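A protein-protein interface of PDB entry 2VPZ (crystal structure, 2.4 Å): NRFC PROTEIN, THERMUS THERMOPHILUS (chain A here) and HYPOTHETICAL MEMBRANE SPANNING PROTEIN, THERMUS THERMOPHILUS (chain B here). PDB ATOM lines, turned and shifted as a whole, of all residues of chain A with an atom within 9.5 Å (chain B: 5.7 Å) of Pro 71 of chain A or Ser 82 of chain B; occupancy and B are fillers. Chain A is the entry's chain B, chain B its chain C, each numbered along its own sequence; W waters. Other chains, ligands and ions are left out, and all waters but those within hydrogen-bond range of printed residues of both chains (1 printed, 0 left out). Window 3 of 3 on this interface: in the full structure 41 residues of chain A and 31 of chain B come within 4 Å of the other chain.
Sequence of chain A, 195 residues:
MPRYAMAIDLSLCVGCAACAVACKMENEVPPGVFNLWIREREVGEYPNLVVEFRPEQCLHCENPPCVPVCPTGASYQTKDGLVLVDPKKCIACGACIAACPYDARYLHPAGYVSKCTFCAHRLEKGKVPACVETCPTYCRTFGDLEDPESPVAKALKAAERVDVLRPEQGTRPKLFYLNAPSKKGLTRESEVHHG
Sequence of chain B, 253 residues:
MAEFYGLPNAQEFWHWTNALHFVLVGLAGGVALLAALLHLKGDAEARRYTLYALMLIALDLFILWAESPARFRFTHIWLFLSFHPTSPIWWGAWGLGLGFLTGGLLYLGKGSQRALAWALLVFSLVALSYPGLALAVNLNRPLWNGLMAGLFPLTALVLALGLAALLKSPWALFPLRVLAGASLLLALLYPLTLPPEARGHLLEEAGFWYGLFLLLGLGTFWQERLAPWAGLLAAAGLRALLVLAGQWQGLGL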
ATOM      1  N   CYS A  66      -3.511 -14.159 -25.034  1.00  0.00           N
ATOM      2  CA  CYS A  66      -3.242 -15.255 -25.954  1.00  0.00           C
ATOM      3  C   CYS A  66      -3.791 -16.615 -25.522  1.00  0.00           C
ATOM      4  O   CYS A  66      -3.763 -17.584 -26.300  1.00  0.00           O
ATOM      5  CB  CYS A  66      -1.738 -15.347 -26.224  1.00  0.00           C
ATOM      6  SG  CYS A  66      -0.750 -15.997 -24.854  1.00  0.00           S
ATOM      7  N   VAL A  67      -4.279 -16.679 -24.284  1.00  0.00           N
ATOM      8  CA  VAL A  67      -4.870 -17.891 -23.698  1.00  0.00           C
ATOM      9  C   VAL A  67      -6.449 -17.976 -23.900  1.00  0.00           C
ATOM     10  O   VAL A  67      -6.896 -18.852 -24.662  1.00  0.00           O
ATOM     11  CB  VAL A  67      -4.391 -18.081 -22.149  1.00  0.00           C
ATOM     12  CG1 VAL A  67      -5.208 -19.186 -21.464  1.00  0.00           C
ATOM     13  CG2 VAL A  67      -2.851 -18.469 -22.066  1.00  0.00           C
ATOM     14  N   PRO A  68      -7.288 -17.069 -23.307  1.00  0.00           N
ATOM     15  CA  PRO A  68      -8.761 -17.173 -23.513  1.00  0.00           C
ATOM     16  C   PRO A  68      -9.362 -17.365 -24.917  1.00  0.00           C
ATOM     17  O   PRO A  68     -10.492 -17.835 -25.087  1.00  0.00           O
ATOM     18  CB  PRO A  68      -9.334 -15.861 -22.928  1.00  0.00           C
ATOM     19  CG  PRO A  68      -8.147 -14.923 -22.792  1.00  0.00           C
ATOM     20  CD  PRO A  68      -6.974 -15.890 -22.485  1.00  0.00           C
ATOM     21  N   VAL A  69      -8.583 -17.011 -25.908  1.00  0.00           N
ATOM     22  CA  VAL A  69      -9.006 -16.958 -27.293  1.00  0.00           C
ATOM     23  C   VAL A  69      -8.817 -18.250 -28.092  1.00  0.00           C
ATOM     24  O   VAL A  69      -9.183 -18.368 -29.263  1.00  0.00           O
ATOM     25  CB  VAL A  69      -8.217 -15.741 -27.857  1.00  0.00           C
ATOM     26  CG1 VAL A  69      -6.939 -16.204 -28.567  1.00  0.00           C
ATOM     27  CG2 VAL A  69      -9.105 -14.847 -28.646  1.00  0.00           C
ATOM     28  N   CYS A  70      -8.269 -19.228 -27.394  1.00  0.00           N
ATOM     29  CA  CYS A  70      -7.945 -20.535 -27.947  1.00  0.00           C
ATOM     30  C   CYS A  70      -9.138 -21.503 -27.839  1.00  0.00           C
ATOM     31  O   CYS A  70      -9.605 -21.783 -26.732  1.00  0.00           O
ATOM     32  CB  CYS A  70      -6.673 -21.066 -27.230  1.00  0.00           C
ATOM     33  SG  CYS A  70      -6.062 -22.732 -27.745  1.00  0.00           S
ATOM     34  N   PRO A  71      -9.595 -22.077 -28.986  1.00  0.00           N
ATOM     35  CA  PRO A  71     -10.745 -22.997 -29.010  1.00  0.00           C
ATOM     36  C   PRO A  71     -10.705 -24.413 -28.401  1.00  0.00           C
ATOM     37  O   PRO A  71     -11.687 -24.919 -27.852  1.00  0.00           O
ATOM     38  CB  PRO A  71     -11.112 -23.021 -30.481  1.00  0.00           C
ATOM     39  CG  PRO A  71      -9.748 -23.097 -31.133  1.00  0.00           C
ATOM     40  CD  PRO A  71      -8.885 -22.129 -30.278  1.00  0.00           C
ATOM     41  N   THR A  72      -9.564 -25.024 -28.574  1.00  0.00           N
ATOM     42  CA  THR A  72      -9.149 -26.347 -28.145  1.00  0.00           C
ATOM     43  C   THR A  72      -8.602 -25.834 -26.799  1.00  0.00           C
ATOM     44  O   THR A  72      -8.836 -24.668 -26.533  1.00  0.00           O
ATOM     45  CB  THR A  72      -8.030 -26.642 -29.164  1.00  0.00           C
ATOM     46  OG1 THR A  72      -8.463 -27.571 -30.147  1.00  0.00           O
ATOM     47  CG2 THR A  72      -6.751 -26.978 -28.471  1.00  0.00           C
ATOM     48  N   GLY A  73      -7.957 -26.601 -25.933  1.00  0.00           N
ATOM     49  CA  GLY A  73      -7.358 -25.955 -24.780  1.00  0.00           C
ATOM     50  C   GLY A  73      -5.807 -25.991 -24.871  1.00  0.00           C
ATOM     51  O   GLY A  73      -5.115 -25.962 -23.844  1.00  0.00           O
ATOM     52  N   ALA A  74      -5.229 -26.066 -26.074  1.00  0.00           N
ATOM     53  CA  ALA A  74      -3.760 -26.160 -26.242  1.00  0.00           C
ATOM     54  C   ALA A  74      -2.925 -25.037 -25.566  1.00  0.00           C
ATOM     55  O   ALA A  74      -1.880 -25.287 -24.942  1.00  0.00           O
ATOM     56  CB  ALA A  74      -3.391 -26.285 -27.756  1.00  0.00           C
ATOM     57  N   SER A  75      -3.408 -23.806 -25.675  1.00  0.00           N
ATOM     58  CA  SER A  75      -2.789 -22.607 -25.080  1.00  0.00           C
ATOM     59  C   SER A  75      -3.132 -22.499 -23.566  1.00  0.00           C
ATOM     60  O   SER A  75      -4.299 -22.323 -23.221  1.00  0.00           O
ATOM     61  CB  SER A  75      -3.294 -21.364 -25.832  1.00  0.00           C
ATOM     62  OG  SER A  75      -2.662 -20.169 -25.437  1.00  0.00           O
ATOM     63  N   LYS A  89      -3.084 -30.750 -28.680  1.00  0.00           N
ATOM     64  CA  LYS A  89      -4.404 -30.161 -28.850  1.00  0.00           C
ATOM     65  C   LYS A  89      -4.416 -29.030 -29.863  1.00  0.00           C
ATOM     66  O   LYS A  89      -5.477 -28.602 -30.323  1.00  0.00           O
ATOM     67  CB  LYS A  89      -4.926 -29.672 -27.519  1.00  0.00           C
ATOM     68  CG  LYS A  89      -4.980 -30.805 -26.574  1.00  0.00           C
ATOM     69  CD  LYS A  89      -5.396 -30.385 -25.235  1.00  0.00           C
ATOM     70  CE  LYS A  89      -6.031 -31.551 -24.546  1.00  0.00           C
ATOM     71  NZ  LYS A  89      -6.762 -31.034 -23.371  1.00  0.00           N
ATOM     72  N   CYS A  90      -3.237 -28.563 -30.240  1.00  0.00           N
ATOM     73  CA  CYS A  90      -3.147 -27.464 -31.191  1.00  0.00           C
ATOM     74  C   CYS A  90      -3.631 -27.779 -32.630  1.00  0.00           C
ATOM     75  O   CYS A  90      -3.196 -28.757 -33.240  1.00  0.00           O
ATOM     76  CB  CYS A  90      -1.730 -26.898 -31.203  1.00  0.00           C
ATOM     77  SG  CYS A  90      -1.674 -25.409 -32.217  1.00  0.00           S
ATOM     78  N   ILE A  91      -4.549 -26.955 -33.144  1.00  0.00           N
ATOM     79  CA  ILE A  91      -5.123 -27.093 -34.499  1.00  0.00           C
ATOM     80  C   ILE A  91      -4.542 -26.050 -35.470  1.00  0.00           C
ATOM     81  O   ILE A  91      -4.982 -25.940 -36.617  1.00  0.00           O
ATOM     82  CB  ILE A  91      -6.739 -27.004 -34.533  1.00  0.00           C
ATOM     83  CG1 ILE A  91      -7.232 -25.583 -34.303  1.00  0.00           C
ATOM     84  CG2 ILE A  91      -7.344 -27.937 -33.468  1.00  0.00           C
ATOM     85  CD1 ILE A  91      -8.757 -25.390 -34.435  1.00  0.00           C
ATOM     86  N   ALA A  92      -3.592 -25.260 -34.982  1.00  0.00           N
ATOM     87  CA  ALA A  92      -2.904 -24.264 -35.801  1.00  0.00           C
ATOM     88  C   ALA A  92      -3.894 -23.294 -36.492  1.00  0.00           C
ATOM     89  O   ALA A  92      -3.801 -23.020 -37.695  1.00  0.00           O
ATOM     90  CB  ALA A  92      -2.020 -25.020 -36.852  1.00  0.00           C
ATOM     91  N   CYS A  93      -4.833 -22.785 -35.703  1.00  0.00           N
ATOM     92  CA  CYS A  93      -5.877 -21.859 -36.158  1.00  0.00           C
ATOM     93  C   CYS A  93      -5.359 -20.400 -36.194  1.00  0.00           C
ATOM     94  O   CYS A  93      -5.920 -19.548 -36.900  1.00  0.00           O
ATOM     95  CB  CYS A  93      -7.144 -21.975 -35.269  1.00  0.00           C
ATOM     96  SG  CYS A  93      -6.903 -21.398 -33.503  1.00  0.00           S
ATOM     97  N   GLY A  94      -4.293 -20.121 -35.445  1.00  0.00           N
ATOM     98  CA  GLY A  94      -3.681 -18.793 -35.419  1.00  0.00           C
ATOM     99  C   GLY A  94      -4.356 -17.695 -34.604  1.00  0.00           C
ATOM    100  O   GLY A  94      -4.031 -16.507 -34.728  1.00  0.00           O
ATOM    101  N   ALA A  95      -5.300 -18.094 -33.761  1.00  0.00           N
ATOM    102  CA  ALA A  95      -6.055 -17.181 -32.912  1.00  0.00           C
ATOM    103  C   ALA A  95      -5.139 -16.473 -31.904  1.00  0.00           C
ATOM    104  O   ALA A  95      -5.288 -15.271 -31.647  1.00  0.00           O
ATOM    105  CB  ALA A  95      -7.192 -17.949 -32.157  1.00  0.00           C
ATOM    106  N   CYS A  96      -4.199 -17.242 -31.356  1.00  0.00           N
ATOM    107  CA  CYS A  96      -3.185 -16.807 -30.370  1.00  0.00           C
ATOM    108  C   CYS A  96      -2.177 -15.807 -30.997  1.00  0.00           C
ATOM    109  O   CYS A  96      -1.686 -14.883 -30.328  1.00  0.00           O
ATOM    110  CB  CYS A  96      -2.471 -18.027 -29.765  1.00  0.00           C
ATOM    111  SG  CYS A  96      -1.844 -19.209 -30.979  1.00  0.00           S
ATOM    112  N   TRP B  78     -10.460 -32.064 -30.474  1.00  0.00           N
ATOM    113  CA  TRP B  78     -10.452 -31.290 -29.204  1.00  0.00           C
ATOM    114  C   TRP B  78     -11.370 -30.073 -29.162  1.00  0.00           C
ATOM    115  O   TRP B  78     -11.721 -29.541 -28.101  1.00  0.00           O
ATOM    116  CB  TRP B  78      -9.021 -30.918 -28.818  1.00  0.00           C
ATOM    117  CG  TRP B  78      -8.229 -32.155 -28.562  1.00  0.00           C
ATOM    118  CD1 TRP B  78      -7.346 -32.769 -29.408  1.00  0.00           C
ATOM    119  CD2 TRP B  78      -8.280 -32.984 -27.379  1.00  0.00           C
ATOM    120  NE1 TRP B  78      -6.848 -33.907 -28.829  1.00  0.00           N
ATOM    121  CE2 TRP B  78      -7.399 -34.066 -27.587  1.00  0.00           C
ATOM    122  CE3 TRP B  78      -8.988 -32.911 -26.161  1.00  0.00           C
ATOM    123  CZ2 TRP B  78      -7.193 -35.077 -26.627  1.00  0.00           C
ATOM    124  CZ3 TRP B  78      -8.785 -33.923 -25.192  1.00  0.00           C
ATOM    125  CH2 TRP B  78      -7.888 -34.990 -25.443  1.00  0.00           C
ATOM    126  N   LEU B  79     -11.766 -29.641 -30.349  1.00  0.00           N
ATOM    127  CA  LEU B  79     -12.710 -28.541 -30.539  1.00  0.00           C
ATOM    128  C   LEU B  79     -14.062 -28.939 -29.860  1.00  0.00           C
ATOM    129  O   LEU B  79     -14.801 -28.100 -29.316  1.00  0.00           O
ATOM    130  CB  LEU B  79     -12.940 -28.343 -32.045  1.00  0.00           C
ATOM    131  CG  LEU B  79     -12.936 -26.949 -32.686  1.00  0.00           C
ATOM    132  CD1 LEU B  79     -12.003 -26.010 -31.903  1.00  0.00           C
ATOM    133  CD2 LEU B  79     -12.515 -27.042 -34.170  1.00  0.00           C
ATOM    134  N   PHE B  80     -14.326 -30.243 -29.909  1.00  0.00           N
ATOM    135  CA  PHE B  80     -15.545 -30.887 -29.433  1.00  0.00           C
ATOM    136  C   PHE B  80     -15.526 -31.669 -28.126  1.00  0.00           C
ATOM    137  O   PHE B  80     -16.553 -32.185 -27.698  1.00  0.00           O
ATOM    138  CB  PHE B  80     -16.088 -31.741 -30.573  1.00  0.00           C
ATOM    139  CG  PHE B  80     -16.437 -30.959 -31.803  1.00  0.00           C
ATOM    140  CD1 PHE B  80     -15.738 -31.125 -33.009  1.00  0.00           C
ATOM    141  CD2 PHE B  80     -17.444 -29.999 -31.733  1.00  0.00           C
ATOM    142  CE1 PHE B  80     -16.044 -30.324 -34.124  1.00  0.00           C
ATOM    143  CE2 PHE B  80     -17.769 -29.191 -32.826  1.00  0.00           C
ATOM    144  CZ  PHE B  80     -17.069 -29.349 -34.028  1.00  0.00           C
ATOM    145  N   LEU B  81     -14.364 -31.761 -27.493  1.00  0.00           N
ATOM    146  CA  LEU B  81     -14.255 -32.469 -26.215  1.00  0.00           C
ATOM    147  C   LEU B  81     -13.926 -31.498 -25.072  1.00  0.00           C
ATOM    148  O   LEU B  81     -13.495 -31.922 -24.011  1.00  0.00           O
ATOM    149  CB  LEU B  81     -13.191 -33.588 -26.272  1.00  0.00           C
ATOM    150  CG  LEU B  81     -13.248 -34.646 -27.391  1.00  0.00           C
ATOM    151  CD1 LEU B  81     -11.833 -35.155 -27.733  1.00  0.00           C
ATOM    152  CD2 LEU B  81     -14.169 -35.813 -27.015  1.00  0.00           C
ATOM    153  N   SER B  82     -14.109 -30.194 -25.284  1.00  0.00           N
ATOM    154  CA  SER B  82     -13.820 -29.237 -24.227  1.00  0.00           C
ATOM    155  C   SER B  82     -14.801 -28.054 -24.243  1.00  0.00           C
ATOM    156  O   SER B  82     -15.615 -27.896 -25.159  1.00  0.00           O
ATOM    157  CB  SER B  82     -12.355 -28.763 -24.297  1.00  0.00           C
ATOM    158  OG  SER B  82     -12.140 -27.881 -25.377  1.00  0.00           O
ATOM    159  N   PHE B  83     -14.693 -27.220 -23.210  1.00  0.00           N
ATOM    160  CA  PHE B  83     -15.559 -26.062 -23.020  1.00  0.00           C
ATOM    161  C   PHE B  83     -14.742 -24.738 -22.974  1.00  0.00           C
ATOM    162  O   PHE B  83     -14.102 -24.460 -21.959  1.00  0.00           O
ATOM    163  CB  PHE B  83     -16.330 -26.302 -21.710  1.00  0.00           C
ATOM    164  CG  PHE B  83     -17.373 -25.274 -21.405  1.00  0.00           C
ATOM    165  CD1 PHE B  83     -18.442 -25.069 -22.272  1.00  0.00           C
ATOM    166  CD2 PHE B  83     -17.289 -24.506 -20.243  1.00  0.00           C
ATOM    167  CE1 PHE B  83     -19.425 -24.106 -21.992  1.00  0.00           C
ATOM    168  CE2 PHE B  83     -18.264 -23.533 -19.944  1.00  0.00           C
ATOM    169  CZ  PHE B  83     -19.333 -23.334 -20.822  1.00  0.00           C
ATOM    170  N   HIS B  84     -14.751 -23.952 -24.054  1.00  0.00           N
ATOM    171  CA  HIS B  84     -14.050 -22.673 -24.098  1.00  0.00           C
ATOM    172  C   HIS B  84     -14.975 -21.535 -24.531  1.00  0.00           C
ATOM    173  O   HIS B  84     -14.886 -21.024 -25.657  1.00  0.00           O
ATOM    174  CB  HIS B  84     -12.748 -22.851 -24.935  1.00  0.00           C
ATOM    175  CG  HIS B  84     -11.787 -23.833 -24.396  1.00  0.00           C
ATOM    176  ND1 HIS B  84     -11.068 -23.598 -23.270  1.00  0.00           N
ATOM    177  CD2 HIS B  84     -11.539 -25.099 -24.737  1.00  0.00           C
ATOM    178  CE1 HIS B  84     -10.421 -24.678 -22.917  1.00  0.00           C
ATOM    179  NE2 HIS B  84     -10.689 -25.616 -23.801  1.00  0.00           N
ATOM    180  N   SER B  87     -13.815 -18.080 -26.205  1.00  0.00           N
ATOM    181  CA  SER B  87     -13.219 -18.136 -27.542  1.00  0.00           C
ATOM    182  C   SER B  87     -14.149 -18.070 -28.796  1.00  0.00           C
ATOM    183  O   SER B  87     -14.918 -19.011 -29.006  1.00  0.00           O
ATOM    184  CB  SER B  87     -12.293 -19.398 -27.619  1.00  0.00           C
ATOM    185  OG  SER B  87     -12.152 -19.910 -28.920  1.00  0.00           O
ATOM    186  N   ILE B  89     -13.816 -18.737 -31.956  1.00  0.00           N
ATOM    187  CA  ILE B  89     -13.665 -19.899 -32.836  1.00  0.00           C
ATOM    188  C   ILE B  89     -14.307 -21.150 -32.223  1.00  0.00           C
ATOM    189  O   ILE B  89     -14.758 -22.039 -32.938  1.00  0.00           O
ATOM    190  CB  ILE B  89     -12.166 -20.204 -33.210  1.00  0.00           C
ATOM    191  CG1 ILE B  89     -11.536 -19.007 -33.922  1.00  0.00           C
ATOM    192  CG2 ILE B  89     -12.085 -21.473 -34.121  1.00  0.00           C
ATOM    193  CD1 ILE B  89     -11.799 -18.953 -35.443  1.00  0.00           C
ATOM    194  N   TRP B  90     -14.348 -21.216 -30.897  1.00  0.00           N
ATOM    195  CA  TRP B  90     -14.991 -22.344 -30.234  1.00  0.00           C
ATOM    196  C   TRP B  90     -16.526 -22.197 -30.461  1.00  0.00           C
ATOM    197  O   TRP B  90     -17.201 -23.167 -30.848  1.00  0.00           O
ATOM    198  CB  TRP B  90     -14.632 -22.375 -28.750  1.00  0.00           C
ATOM    199  CG  TRP B  90     -15.232 -23.520 -28.020  1.00  0.00           C
ATOM    200  CD1 TRP B  90     -14.705 -24.783 -27.841  1.00  0.00           C
ATOM    201  CD2 TRP B  90     -16.505 -23.528 -27.361  1.00  0.00           C
ATOM    202  NE1 TRP B  90     -15.581 -25.560 -27.110  1.00  0.00           N
ATOM    203  CE2 TRP B  90     -16.690 -24.820 -26.805  1.00  0.00           C
ATOM    204  CE3 TRP B  90     -17.521 -22.567 -27.192  1.00  0.00           C
ATOM    205  CZ2 TRP B  90     -17.852 -25.172 -26.076  1.00  0.00           C
ATOM    206  CZ3 TRP B  90     -18.685 -22.909 -26.467  1.00  0.00           C
ATOM    207  CH2 TRP B  90     -18.835 -24.206 -25.921  1.00  0.00           C
ATOM    208  N   TRP B  94     -19.175 -25.021 -32.657  1.00  0.00           N
ATOM    209  CA  TRP B  94     -20.391 -25.589 -32.109  1.00  0.00           C
ATOM    210  C   TRP B  94     -21.703 -25.102 -32.811  1.00  0.00           C
ATOM    211  O   TRP B  94     -22.607 -25.911 -33.004  1.00  0.00           O
ATOM    212  CB  TRP B  94     -20.410 -25.386 -30.578  1.00  0.00           C
ATOM    213  CG  TRP B  94     -19.483 -26.369 -29.837  1.00  0.00           C
ATOM    214  CD1 TRP B  94     -18.127 -26.239 -29.611  1.00  0.00           C
ATOM    215  CD2 TRP B  94     -19.860 -27.631 -29.249  1.00  0.00           C
ATOM    216  NE1 TRP B  94     -17.657 -27.338 -28.925  1.00  0.00           N
ATOM    217  CE2 TRP B  94     -18.692 -28.206 -28.692  1.00  0.00           C
ATOM    218  CE3 TRP B  94     -21.076 -28.333 -29.150  1.00  0.00           C
ATOM    219  CZ2 TRP B  94     -18.704 -29.458 -28.028  1.00  0.00           C
ATOM    220  CZ3 TRP B  94     -21.093 -29.583 -28.488  1.00  0.00           C
ATOM    221  CH2 TRP B  94     -19.906 -30.127 -27.940  1.00  0.00           C
HETATM  222  O   HOH W   1     -11.124 -17.151 -31.124  1.00  0.00           O
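The side-chain hydroxyl (OG) of Ser 87 of chain B lies within hydrogen-bond range of the backbone carbonyl oxygen (O) of Val 69 of chain A (3.4 Å). The backbone carbonyl oxygen (O) of Thr 72 of chain A lies close to a ring nitrogen (NE2) of His 84 of chain B (3.4 Å). The backbone nitrogen of Pro 71 of chain A lies close to the side-chain hydroxyl of Ser 87 of chain B.
The backbone NH (N) of Ser 75 of chain A sits close to the side-chain sulfur (SG) of Cys 70 of chain A (3.5 Å). OG1 of Thr 72 of chain A lies close to O of Lys 89 of chain A (3.2 Å). The side-chain hydroxyl of Ser 82 of chain B sits at hydrogen-bond distance from the backbone carbonyl oxygen of Trp 78 of chain B (3.2 Å). O of Leu 79 of chain B sits at hydrogen-bond distance from NE1 of Trp 94 of chain B (3.0 Å). The indole nitrogen of Trp 90 of chain B sits at hydrogen-bond distance from the backbone carbonyl oxygen of Ser 82 of chain B. OG of Ser 87 of chain B sits at hydrogen-bond distance from N of Trp 90 of chain B, 3.2 Å away.
Among the printed residues, pairs that only touch across the chains: Pro 68 of chain A with Ser 87 of chain B, Cys 70 of chain A with His 84 of chain B, Cys 70 of chain A with Ser 87 of chain B, Pro 71 of chain A with Leu 79 of chain B, Pro 71 of chain A with Ser 82 of chain B, Pro 71 of chain A with His 84 of chain B, Pro 71 of chain A with Trp 90 of chain B, Thr 72 of chain A with Trp 78 of chain B, Thr 72 of chain A with Leu 79 of chain B, Gly 73 of chain A with His 84 of chain B and Lys 89 of chain A with Trp 78 of chain B.
Ser 82 of chain B touches just one residue of chain A: Pro 71. Of the printed residues of chain B, Thr 72 of chain A touches Trp 78 (3.6 Å), Leu 79 (3.9 Å) and His 84 (3.3 Å). Printed residues of chain B within 4 Å of Val 69 of chain A: Ser 87 (3.4 Å). Of the printed residues of chain B, Lys 89 of chain A touches Trp 78 (3.6 Å). Ala 74 of chain A touches none of the printed residues of chain B. Trp 94 of chain B touches none of the printed residues of chain A.
Printed residues of chain B that touch a printed residue of chain A: Trp 78, Leu 79, Ser 82, His 84, Ser 87 and Trp 90. Of the 18 printed residues of chain A, 7 touch a printed residue of chain B. Among the printed residues, 14 pairs touch across the chains. Among the printed residues, no Asp or Glu carboxylate lies within 4 Å of a Lys or Arg side-chain nitrogen of the other chain.
Water W1 lies within hydrogen-bond range of O of Val 69 of chain A (3.0 Å) and N of Ile 89 of chain B (3.2 Å).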
